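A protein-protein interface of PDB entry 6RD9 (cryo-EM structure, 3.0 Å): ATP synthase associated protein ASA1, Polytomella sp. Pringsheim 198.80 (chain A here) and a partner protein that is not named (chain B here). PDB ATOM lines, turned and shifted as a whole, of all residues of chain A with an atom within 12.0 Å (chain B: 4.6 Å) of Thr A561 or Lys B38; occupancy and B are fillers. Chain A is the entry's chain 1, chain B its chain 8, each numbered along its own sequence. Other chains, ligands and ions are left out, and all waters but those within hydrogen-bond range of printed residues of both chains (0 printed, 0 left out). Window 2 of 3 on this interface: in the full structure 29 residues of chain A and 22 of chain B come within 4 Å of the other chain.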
ATOM      1  N   LEU A 552      18.946   5.948 -20.659  1.00  0.00           N
ATOM      2  CA  LEU A 552      20.362   6.272 -20.651  1.00  0.00           C
ATOM      3  C   LEU A 552      20.555   7.737 -20.368  1.00  0.00           C
ATOM      4  O   LEU A 552      21.433   8.116 -19.599  1.00  0.00           O
ATOM      5  CB  LEU A 552      21.002   5.920 -21.979  1.00  0.00           C
ATOM      6  CG  LEU A 552      22.475   6.245 -22.091  1.00  0.00           C
ATOM      7  CD1 LEU A 552      23.252   5.432 -21.138  1.00  0.00           C
ATOM      8  CD2 LEU A 552      22.953   6.012 -23.449  1.00  0.00           C
ATOM      9  N   ILE A 553      19.722   8.571 -20.970  1.00  0.00           N
ATOM     10  CA  ILE A 553      19.703   9.996 -20.702  1.00  0.00           C
ATOM     11  C   ILE A 553      19.276  10.271 -19.275  1.00  0.00           C
ATOM     12  O   ILE A 553      19.798  11.178 -18.641  1.00  0.00           O
ATOM     13  CB  ILE A 553      18.785  10.648 -21.742  1.00  0.00           C
ATOM     14  CG1 ILE A 553      19.391  10.497 -23.123  1.00  0.00           C
ATOM     15  CG2 ILE A 553      18.496  12.050 -21.447  1.00  0.00           C
ATOM     16  CD1 ILE A 553      20.765  10.992 -23.244  1.00  0.00           C
ATOM     17  N   LYS A 554      18.377   9.466 -18.726  1.00  0.00           N
ATOM     18  CA  LYS A 554      17.939   9.619 -17.347  1.00  0.00           C
ATOM     19  C   LYS A 554      19.057   9.331 -16.365  1.00  0.00           C
ATOM     20  O   LYS A 554      19.180  10.010 -15.351  1.00  0.00           O
ATOM     21  CB  LYS A 554      16.770   8.691 -17.079  1.00  0.00           C
ATOM     22  CG  LYS A 554      16.162   8.826 -15.730  1.00  0.00           C
ATOM     23  CD  LYS A 554      15.519   7.561 -15.324  1.00  0.00           C
ATOM     24  CE  LYS A 554      14.924   7.679 -13.983  1.00  0.00           C
ATOM     25  NZ  LYS A 554      14.486   6.355 -13.527  1.00  0.00           N
ATOM     26  N   LYS A 555      19.881   8.333 -16.647  1.00  0.00           N
ATOM     27  CA  LYS A 555      20.988   7.999 -15.769  1.00  0.00           C
ATOM     28  C   LYS A 555      22.183   8.903 -15.972  1.00  0.00           C
ATOM     29  O   LYS A 555      22.976   9.066 -15.055  1.00  0.00           O
ATOM     30  CB  LYS A 555      21.424   6.570 -16.001  1.00  0.00           C
ATOM     31  CG  LYS A 555      20.434   5.560 -15.630  1.00  0.00           C
ATOM     32  CD  LYS A 555      20.986   4.221 -15.865  1.00  0.00           C
ATOM     33  CE  LYS A 555      19.970   3.329 -16.406  1.00  0.00           C
ATOM     34  NZ  LYS A 555      20.375   1.954 -16.199  1.00  0.00           N
ATOM     35  N   ILE A 556      22.377   9.429 -17.174  1.00  0.00           N
ATOM     36  CA  ILE A 556      23.407  10.432 -17.408  1.00  0.00           C
ATOM     37  C   ILE A 556      23.069  11.712 -16.673  1.00  0.00           C
ATOM     38  O   ILE A 556      23.929  12.321 -16.039  1.00  0.00           O
ATOM     39  CB  ILE A 556      23.566  10.669 -18.916  1.00  0.00           C
ATOM     40  CG1 ILE A 556      24.383   9.568 -19.557  1.00  0.00           C
ATOM     41  CG2 ILE A 556      24.231  11.938 -19.192  1.00  0.00           C
ATOM     42  CD1 ILE A 556      24.265   9.572 -21.005  1.00  0.00           C
ATOM     43  N   ASP A 557      21.805  12.114 -16.708  1.00  0.00           N
ATOM     44  CA  ASP A 557      21.348  13.286 -15.984  1.00  0.00           C
ATOM     45  C   ASP A 557      21.413  13.121 -14.489  1.00  0.00           C
ATOM     46  O   ASP A 557      21.370  14.115 -13.780  1.00  0.00           O
ATOM     47  CB  ASP A 557      19.912  13.604 -16.340  1.00  0.00           C
ATOM     48  CG  ASP A 557      19.764  14.123 -17.713  1.00  0.00           C
ATOM     49  OD1 ASP A 557      20.773  14.202 -18.420  1.00  0.00           O
ATOM     50  OD2 ASP A 557      18.636  14.464 -18.089  1.00  0.00           O
ATOM     51  N   TRP A 558      21.447  11.901 -13.984  1.00  0.00           N
ATOM     52  CA  TRP A 558      21.611  11.723 -12.554  1.00  0.00           C
ATOM     53  C   TRP A 558      23.016  12.074 -12.129  1.00  0.00           C
ATOM     54  O   TRP A 558      23.222  12.572 -11.029  1.00  0.00           O
ATOM     55  CB  TRP A 558      21.274  10.298 -12.144  1.00  0.00           C
ATOM     56  CG  TRP A 558      21.298  10.092 -10.682  1.00  0.00           C
ATOM     57  CD1 TRP A 558      20.270  10.226  -9.841  1.00  0.00           C
ATOM     58  CD2 TRP A 558      22.424   9.725  -9.887  1.00  0.00           C
ATOM     59  NE1 TRP A 558      20.670   9.971  -8.568  1.00  0.00           N
ATOM     60  CE2 TRP A 558      21.996   9.654  -8.583  1.00  0.00           C
ATOM     61  CE3 TRP A 558      23.755   9.451 -10.164  1.00  0.00           C
ATOM     62  CZ2 TRP A 558      22.839   9.349  -7.563  1.00  0.00           C
ATOM     63  CZ3 TRP A 558      24.574   9.150  -9.169  1.00  0.00           C
ATOM     64  CH2 TRP A 558      24.130   9.096  -7.881  1.00  0.00           C
ATOM     65  N   GLU A 559      23.999  11.804 -12.969  1.00  0.00           N
ATOM     66  CA  GLU A 559      25.364  12.146 -12.620  1.00  0.00           C
ATOM     67  C   GLU A 559      25.587  13.641 -12.666  1.00  0.00           C
ATOM     68  O   GLU A 559      26.356  14.174 -11.874  1.00  0.00           O
ATOM     69  CB  GLU A 559      26.318  11.456 -13.559  1.00  0.00           C
ATOM     70  CG  GLU A 559      26.052  10.035 -13.699  1.00  0.00           C
ATOM     71  CD  GLU A 559      27.189   9.320 -14.321  1.00  0.00           C
ATOM     72  OE1 GLU A 559      28.288   9.875 -14.332  1.00  0.00           O
ATOM     73  OE2 GLU A 559      26.995   8.204 -14.812  1.00  0.00           O
ATOM     74  N   THR A 560      24.954  14.336 -13.598  1.00  0.00           N
ATOM     75  CA  THR A 560      25.086  15.781 -13.633  1.00  0.00           C
ATOM     76  C   THR A 560      24.355  16.420 -12.471  1.00  0.00           C
ATOM     77  O   THR A 560      24.843  17.383 -11.892  1.00  0.00           O
ATOM     78  CB  THR A 560      24.571  16.325 -14.954  1.00  0.00           C
ATOM     79  OG1 THR A 560      25.125  15.561 -16.018  1.00  0.00           O
ATOM     80  CG2 THR A 560      24.996  17.712 -15.142  1.00  0.00           C
ATOM     81  N   THR A 561      23.201  15.881 -12.100  1.00  0.00           N
ATOM     82  CA  THR A 561      22.438  16.444 -10.997  1.00  0.00           C
ATOM     83  C   THR A 561      23.142  16.227  -9.680  1.00  0.00           C
ATOM     84  O   THR A 561      23.205  17.125  -8.843  1.00  0.00           O
ATOM     85  CB  THR A 561      21.062  15.817 -10.963  1.00  0.00           C
ATOM     86  OG1 THR A 561      20.437  16.012 -12.224  1.00  0.00           O
ATOM     87  CG2 THR A 561      20.219  16.435  -9.930  1.00  0.00           C
ATOM     88  N   ASN A 562      23.719  15.053  -9.499  1.00  0.00           N
ATOM     89  CA  ASN A 562      24.368  14.682  -8.259  1.00  0.00           C
ATOM     90  C   ASN A 562      25.860  14.849  -8.319  1.00  0.00           C
ATOM     91  O   ASN A 562      26.582  14.046  -7.739  1.00  0.00           O
ATOM     92  CB  ASN A 562      24.008  13.259  -7.906  1.00  0.00           C
ATOM     93  CG  ASN A 562      22.577  13.130  -7.623  1.00  0.00           C
ATOM     94  OD1 ASN A 562      21.786  12.973  -8.520  1.00  0.00           O
ATOM     95  ND2 ASN A 562      22.210  13.252  -6.376  1.00  0.00           N
ATOM     96  N   ALA A 563      26.318  15.843  -9.065  1.00  0.00           N
ATOM     97  CA  ALA A 563      27.659  16.399  -9.011  1.00  0.00           C
ATOM     98  C   ALA A 563      28.737  15.400  -9.352  1.00  0.00           C
ATOM     99  O   ALA A 563      29.873  15.544  -8.919  1.00  0.00           O
ATOM    100  CB  ALA A 563      27.935  17.011  -7.646  1.00  0.00           C
ATOM    101  N   LEU A 564      28.403  14.373 -10.104  1.00  0.00           N
ATOM    102  CA  LEU A 564      29.355  13.373 -10.542  1.00  0.00           C
ATOM    103  C   LEU A 564      29.501  13.411 -12.046  1.00  0.00           C
ATOM    104  O   LEU A 564      29.641  12.380 -12.685  1.00  0.00           O
ATOM    105  CB  LEU A 564      28.924  11.979 -10.124  1.00  0.00           C
ATOM    106  CG  LEU A 564      28.689  11.604  -8.679  1.00  0.00           C
ATOM    107  CD1 LEU A 564      27.899  10.363  -8.693  1.00  0.00           C
ATOM    108  CD2 LEU A 564      29.988  11.349  -8.028  1.00  0.00           C
ATOM    109  N   GLU A 565      29.476  14.604 -12.633  1.00  0.00           N
ATOM    110  CA  GLU A 565      29.576  14.711 -14.078  1.00  0.00           C
ATOM    111  C   GLU A 565      30.958  14.370 -14.590  1.00  0.00           C
ATOM    112  O   GLU A 565      31.141  14.223 -15.795  1.00  0.00           O
ATOM    113  CB  GLU A 565      29.196  16.106 -14.549  1.00  0.00           C
ATOM    114  CG  GLU A 565      30.168  17.162 -14.157  1.00  0.00           C
ATOM    115  CD  GLU A 565      29.790  17.843 -12.883  1.00  0.00           C
ATOM    116  OE1 GLU A 565      28.825  17.399 -12.245  1.00  0.00           O
ATOM    117  OE2 GLU A 565      30.463  18.813 -12.498  1.00  0.00           O
ATOM    118  N   ASP A 566      31.937  14.241 -13.719  1.00  0.00           N
ATOM    119  CA  ASP A 566      33.256  13.786 -14.098  1.00  0.00           C
ATOM    120  C   ASP A 566      33.566  12.415 -13.530  1.00  0.00           C
ATOM    121  O   ASP A 566      34.719  12.129 -13.235  1.00  0.00           O
ATOM    122  CB  ASP A 566      34.299  14.785 -13.633  1.00  0.00           C
ATOM    123  CG  ASP A 566      34.247  15.023 -12.155  1.00  0.00           C
ATOM    124  OD1 ASP A 566      33.147  15.031 -11.586  1.00  0.00           O
ATOM    125  OD2 ASP A 566      35.313  15.209 -11.551  1.00  0.00           O
ATOM    126  N   PHE A 567      32.560  11.555 -13.374  1.00  0.00           N
ATOM    127  CA  PHE A 567      32.789  10.293 -12.686  1.00  0.00           C
ATOM    128  C   PHE A 567      33.628   9.343 -13.508  1.00  0.00           C
ATOM    129  O   PHE A 567      34.406   8.580 -12.947  1.00  0.00           O
ATOM    130  CB  PHE A 567      31.479   9.621 -12.321  1.00  0.00           C
ATOM    131  CG  PHE A 567      31.646   8.450 -11.415  1.00  0.00           C
ATOM    132  CD1 PHE A 567      32.258   8.597 -10.192  1.00  0.00           C
ATOM    133  CD2 PHE A 567      31.187   7.207 -11.776  1.00  0.00           C
ATOM    134  CE1 PHE A 567      32.418   7.525  -9.354  1.00  0.00           C
ATOM    135  CE2 PHE A 567      31.345   6.140 -10.947  1.00  0.00           C
ATOM    136  CZ  PHE A 567      31.955   6.298  -9.734  1.00  0.00           C
ATOM    137  N   TRP A 583      30.843   0.769 -14.759  1.00  0.00           N
ATOM    138  CA  TRP A 583      30.086   2.003 -14.885  1.00  0.00           C
ATOM    139  C   TRP A 583      29.385   2.066 -16.220  1.00  0.00           C
ATOM    140  O   TRP A 583      28.225   2.464 -16.294  1.00  0.00           O
ATOM    141  CB  TRP A 583      31.006   3.201 -14.707  1.00  0.00           C
ATOM    142  CG  TRP A 583      30.447   4.501 -15.163  1.00  0.00           C
ATOM    143  CD1 TRP A 583      29.608   5.310 -14.484  1.00  0.00           C
ATOM    144  CD2 TRP A 583      30.711   5.151 -16.394  1.00  0.00           C
ATOM    145  NE1 TRP A 583      29.312   6.407 -15.217  1.00  0.00           N
ATOM    146  CE2 TRP A 583      29.982   6.328 -16.403  1.00  0.00           C
ATOM    147  CE3 TRP A 583      31.480   4.833 -17.506  1.00  0.00           C
ATOM    148  CZ2 TRP A 583      30.010   7.197 -17.461  1.00  0.00           C
ATOM    149  CZ3 TRP A 583      31.504   5.690 -18.540  1.00  0.00           C
ATOM    150  CH2 TRP A 583      30.787   6.864 -18.514  1.00  0.00           C
ATOM    151  N   ASN A 587      25.021   1.381 -16.956  1.00  0.00           N
ATOM    152  CA  ASN A 587      24.268   2.470 -17.539  1.00  0.00           C
ATOM    153  C   ASN A 587      23.551   2.064 -18.794  1.00  0.00           C
ATOM    154  O   ASN A 587      22.644   2.770 -19.228  1.00  0.00           O
ATOM    155  CB  ASN A 587      25.177   3.643 -17.866  1.00  0.00           C
ATOM    156  CG  ASN A 587      25.416   4.531 -16.692  1.00  0.00           C
ATOM    157  OD1 ASN A 587      26.217   5.438 -16.752  1.00  0.00           O
ATOM    158  ND2 ASN A 587      24.721   4.275 -15.610  1.00  0.00           N
ATOM    159  N   HIS B  26      17.134  18.745 -18.867  1.00  0.00           N
ATOM    160  CA  HIS B  26      17.741  18.387 -17.618  1.00  0.00           C
ATOM    161  C   HIS B  26      16.920  18.993 -16.485  1.00  0.00           C
ATOM    162  O   HIS B  26      16.224  19.984 -16.689  1.00  0.00           O
ATOM    163  CB  HIS B  26      19.169  18.892 -17.574  1.00  0.00           C
ATOM    164  CG  HIS B  26      19.953  18.334 -16.448  1.00  0.00           C
ATOM    165  ND1 HIS B  26      20.549  17.106 -16.498  1.00  0.00           N
ATOM    166  CD2 HIS B  26      20.172  18.802 -15.208  1.00  0.00           C
ATOM    167  CE1 HIS B  26      21.135  16.861 -15.346  1.00  0.00           C
ATOM    168  NE2 HIS B  26      20.915  17.875 -14.543  1.00  0.00           N
ATOM    169  N   PRO B  27      16.945  18.398 -15.294  1.00  0.00           N
ATOM    170  CA  PRO B  27      16.295  19.029 -14.142  1.00  0.00           C
ATOM    171  C   PRO B  27      16.804  20.408 -13.779  1.00  0.00           C
ATOM    172  O   PRO B  27      16.088  21.144 -13.108  1.00  0.00           O
ATOM    173  CB  PRO B  27      16.574  18.031 -13.030  1.00  0.00           C
ATOM    174  CG  PRO B  27      16.534  16.771 -13.714  1.00  0.00           C
ATOM    175  CD  PRO B  27      17.100  16.959 -15.063  1.00  0.00           C
ATOM    176  N   PHE B  28      18.003  20.782 -14.198  1.00  0.00           N
ATOM    177  CA  PHE B  28      18.560  22.095 -13.943  1.00  0.00           C
ATOM    178  C   PHE B  28      18.080  23.107 -14.955  1.00  0.00           C
ATOM    179  O   PHE B  28      17.989  24.292 -14.645  1.00  0.00           O
ATOM    180  CB  PHE B  28      20.076  22.044 -14.001  1.00  0.00           C
ATOM    181  CG  PHE B  28      20.718  21.288 -12.894  1.00  0.00           C
ATOM    182  CD1 PHE B  28      20.034  20.944 -11.761  1.00  0.00           C
ATOM    183  CD2 PHE B  28      22.042  20.971 -12.972  1.00  0.00           C
ATOM    184  CE1 PHE B  28      20.645  20.277 -10.769  1.00  0.00           C
ATOM    185  CE2 PHE B  28      22.641  20.313 -11.974  1.00  0.00           C
ATOM    186  CZ  PHE B  28      21.944  19.980 -10.872  1.00  0.00           C
ATOM    187  N   THR B  34      16.017  23.815  -8.497  1.00  0.00           N
ATOM    188  CA  THR B  34      16.715  22.541  -8.423  1.00  0.00           C
ATOM    189  C   THR B  34      18.200  22.731  -8.617  1.00  0.00           C
ATOM    190  O   THR B  34      18.993  22.025  -8.003  1.00  0.00           O
ATOM    191  CB  THR B  34      16.193  21.588  -9.482  1.00  0.00           C
ATOM    192  OG1 THR B  34      14.772  21.679  -9.518  1.00  0.00           O
ATOM    193  CG2 THR B  34      16.562  20.185  -9.152  1.00  0.00           C
ATOM    194  N   TYR B  35      18.595  23.677  -9.466  1.00  0.00           N
ATOM    195  CA  TYR B  35      20.002  23.979  -9.623  1.00  0.00           C
ATOM    196  C   TYR B  35      20.558  24.596  -8.366  1.00  0.00           C
ATOM    197  O   TYR B  35      21.647  24.229  -7.929  1.00  0.00           O
ATOM    198  CB  TYR B  35      20.222  24.925 -10.787  1.00  0.00           C
ATOM    199  CG  TYR B  35      21.655  25.344 -10.902  1.00  0.00           C
ATOM    200  CD1 TYR B  35      22.644  24.406 -11.006  1.00  0.00           C
ATOM    201  CD2 TYR B  35      22.016  26.666 -10.897  1.00  0.00           C
ATOM    202  CE1 TYR B  35      23.910  24.753 -11.082  1.00  0.00           C
ATOM    203  CE2 TYR B  35      23.314  27.020 -10.993  1.00  0.00           C
ATOM    204  CZ  TYR B  35      24.249  26.054 -11.092  1.00  0.00           C
ATOM    205  OH  TYR B  35      25.566  26.368 -11.173  1.00  0.00           O
ATOM    206  N   ALA B  36      19.823  25.537  -7.776  1.00  0.00           N
ATOM    207  CA  ALA B  36      20.324  26.276  -6.635  1.00  0.00           C
ATOM    208  C   ALA B  36      20.487  25.400  -5.425  1.00  0.00           C
ATOM    209  O   ALA B  36      21.485  25.506  -4.726  1.00  0.00           O
ATOM    210  CB  ALA B  36      19.404  27.426  -6.298  1.00  0.00           C
ATOM    211  N   THR B  37      19.557  24.504  -5.181  1.00  0.00           N
ATOM    212  CA  THR B  37      19.602  23.728  -3.962  1.00  0.00           C
ATOM    213  C   THR B  37      20.377  22.439  -4.088  1.00  0.00           C
ATOM    214  O   THR B  37      20.877  21.945  -3.081  1.00  0.00           O
ATOM    215  CB  THR B  37      18.188  23.433  -3.502  1.00  0.00           C
ATOM    216  OG1 THR B  37      17.464  22.862  -4.586  1.00  0.00           O
ATOM    217  CG2 THR B  37      17.531  24.710  -3.141  1.00  0.00           C
ATOM    218  N   LYS B  38      20.508  21.884  -5.286  1.00  0.00           N
ATOM    219  CA  LYS B  38      21.277  20.666  -5.467  1.00  0.00           C
ATOM    220  C   LYS B  38      22.667  20.897  -6.013  1.00  0.00           C
ATOM    221  O   LYS B  38      23.526  20.037  -5.830  1.00  0.00           O
ATOM    222  CB  LYS B  38      20.560  19.705  -6.407  1.00  0.00           C
ATOM    223  CG  LYS B  38      19.241  19.245  -5.908  1.00  0.00           C
ATOM    224  CD  LYS B  38      18.880  17.912  -6.492  1.00  0.00           C
ATOM    225  CE  LYS B  38      17.518  17.485  -6.001  1.00  0.00           C
ATOM    226  NZ  LYS B  38      17.171  16.103  -6.416  1.00  0.00           N
ATOM    227  N   LYS B  39      22.907  21.981  -6.681  1.00  0.00           N
ATOM    228  CA  LYS B  39      24.262  22.133  -7.167  1.00  0.00           C
ATOM    229  C   LYS B  39      24.898  23.452  -6.806  1.00  0.00           C
ATOM    230  O   LYS B  39      26.049  23.462  -6.409  1.00  0.00           O
ATOM    231  CB  LYS B  39      24.305  21.966  -8.655  1.00  0.00           C
ATOM    232  CG  LYS B  39      25.669  22.041  -9.220  1.00  0.00           C
ATOM    233  CD  LYS B  39      25.695  21.473 -10.548  1.00  0.00           C
ATOM    234  CE  LYS B  39      26.028  20.058 -10.489  1.00  0.00           C
ATOM    235  NZ  LYS B  39      27.426  19.941 -10.135  1.00  0.00           N
ATOM    236  N   LEU B  40      24.178  24.558  -6.904  1.00  0.00           N
ATOM    237  CA  LEU B  40      24.806  25.857  -6.730  1.00  0.00           C
ATOM    238  C   LEU B  40      25.201  26.098  -5.288  1.00  0.00           C
ATOM    239  O   LEU B  40      26.290  26.594  -5.015  1.00  0.00           O
ATOM    240  CB  LEU B  40      23.876  26.948  -7.217  1.00  0.00           C
ATOM    241  CG  LEU B  40      24.246  28.393  -7.011  1.00  0.00           C
ATOM    242  CD1 LEU B  40      25.507  28.695  -7.734  1.00  0.00           C
ATOM    243  CD2 LEU B  40      23.142  29.228  -7.540  1.00  0.00           C
ATOM    244  N   PRO B  42      25.244  23.521  -2.582  1.00  0.00           N
ATOM    245  CA  PRO B  42      26.163  22.524  -2.023  1.00  0.00           C
ATOM    246  C   PRO B  42      27.544  22.507  -2.632  1.00  0.00           C
ATOM    247  O   PRO B  42      28.502  22.185  -1.927  1.00  0.00           O
ATOM    248  CB  PRO B  42      25.437  21.209  -2.287  1.00  0.00           C
ATOM    249  CG  PRO B  42      24.101  21.572  -2.316  1.00  0.00           C
ATOM    250  CD  PRO B  42      24.033  22.826  -3.031  1.00  0.00           C
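OD1 of Asp A557 lies close to ND1 of His B26, at 3.5 Å.
A ring nitrogen (NE2) of His B26 sits at hydrogen-bond distance from the side-chain hydroxyl (OG1) of Thr A561.
The side-chain amino group of Lys B39 lies within salt-bridge range of the side-chain carboxylate of Glu A565 (3.6 Å).
The backbone carbonyl oxygen (O) of Glu A559 is in hydrogen-bond range of the backbone NH (N) of Glu A565.
O of Asp A557 sits at hydrogen-bond distance from OG1 of Thr A561 (2.6 Å).
The side-chain hydroxyl of Thr A560 sits at hydrogen-bond distance from the backbone carbonyl oxygen of Ile A556, 3.5 Å away.
Thr A560 touches His B26 (CB to CE1, 3.5 Å).
CE2 of Phe B28 touches O of Thr A560, 3.7 Å away.
O of Thr A560 touches CE of Lys B39, 3.2 Å away.
Phe B28 touches Thr A561.
Thr A561 touches Lys B38 (CG2 to CD, 3.97 Å).
NZ of Lys B39 touches CA of Ala A563, 3.7 Å away.
Of chain B, only His B26 (3.0 Å), Phe B28 (3.6 Å) and Lys B38 (3.97 Å) come within 4 Å of Thr A561.
Lys B38 touches just one residue of chain A: Thr A561 (3.97 Å).
No residue of chain A comes within 4 Å of Pro B27.
No residue of chain A comes within 4 Å of Thr B37.
Of chain A, only Thr A560, Ala A563 and Glu A565 come within 4 Å of Lys B39.
Printed residues of chain B within 4 Å of Ala A563: Lys B39.
Of the printed residues of chain B, Asp A557 touches His B26.
Of the printed residues of chain B, Thr A560 touches His B26 (3.5 Å), Phe B28 (3.7 Å) and Lys B39 (3.2 Å).
Of the printed residues of chain A, Phe B28 touches Thr A560 and Thr A561.
The nearest residue of chain A that does not touch Lys B38 is Ala A563 (5.6 Å).
The nearest printed residue of chain B that does not touch Asp A557 is Pro B27 (4.2 Å).
Of the 18 printed residues of chain A, 5 touch a printed residue of chain B.
Along chain A the printed residues that touch a printed residue of chain B span positions 557 to 565.
Of the 11 printed residues of chain B, 4 touch a printed residue of chain A.
Among the printed residues, 9 pairs touch across the chains.
Among the printed residues, Asp or Glu carboxylates within 4 Å of a Lys or Arg side-chain nitrogen of the other chain: Glu A565 with Lys B39 (3.6 Å).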
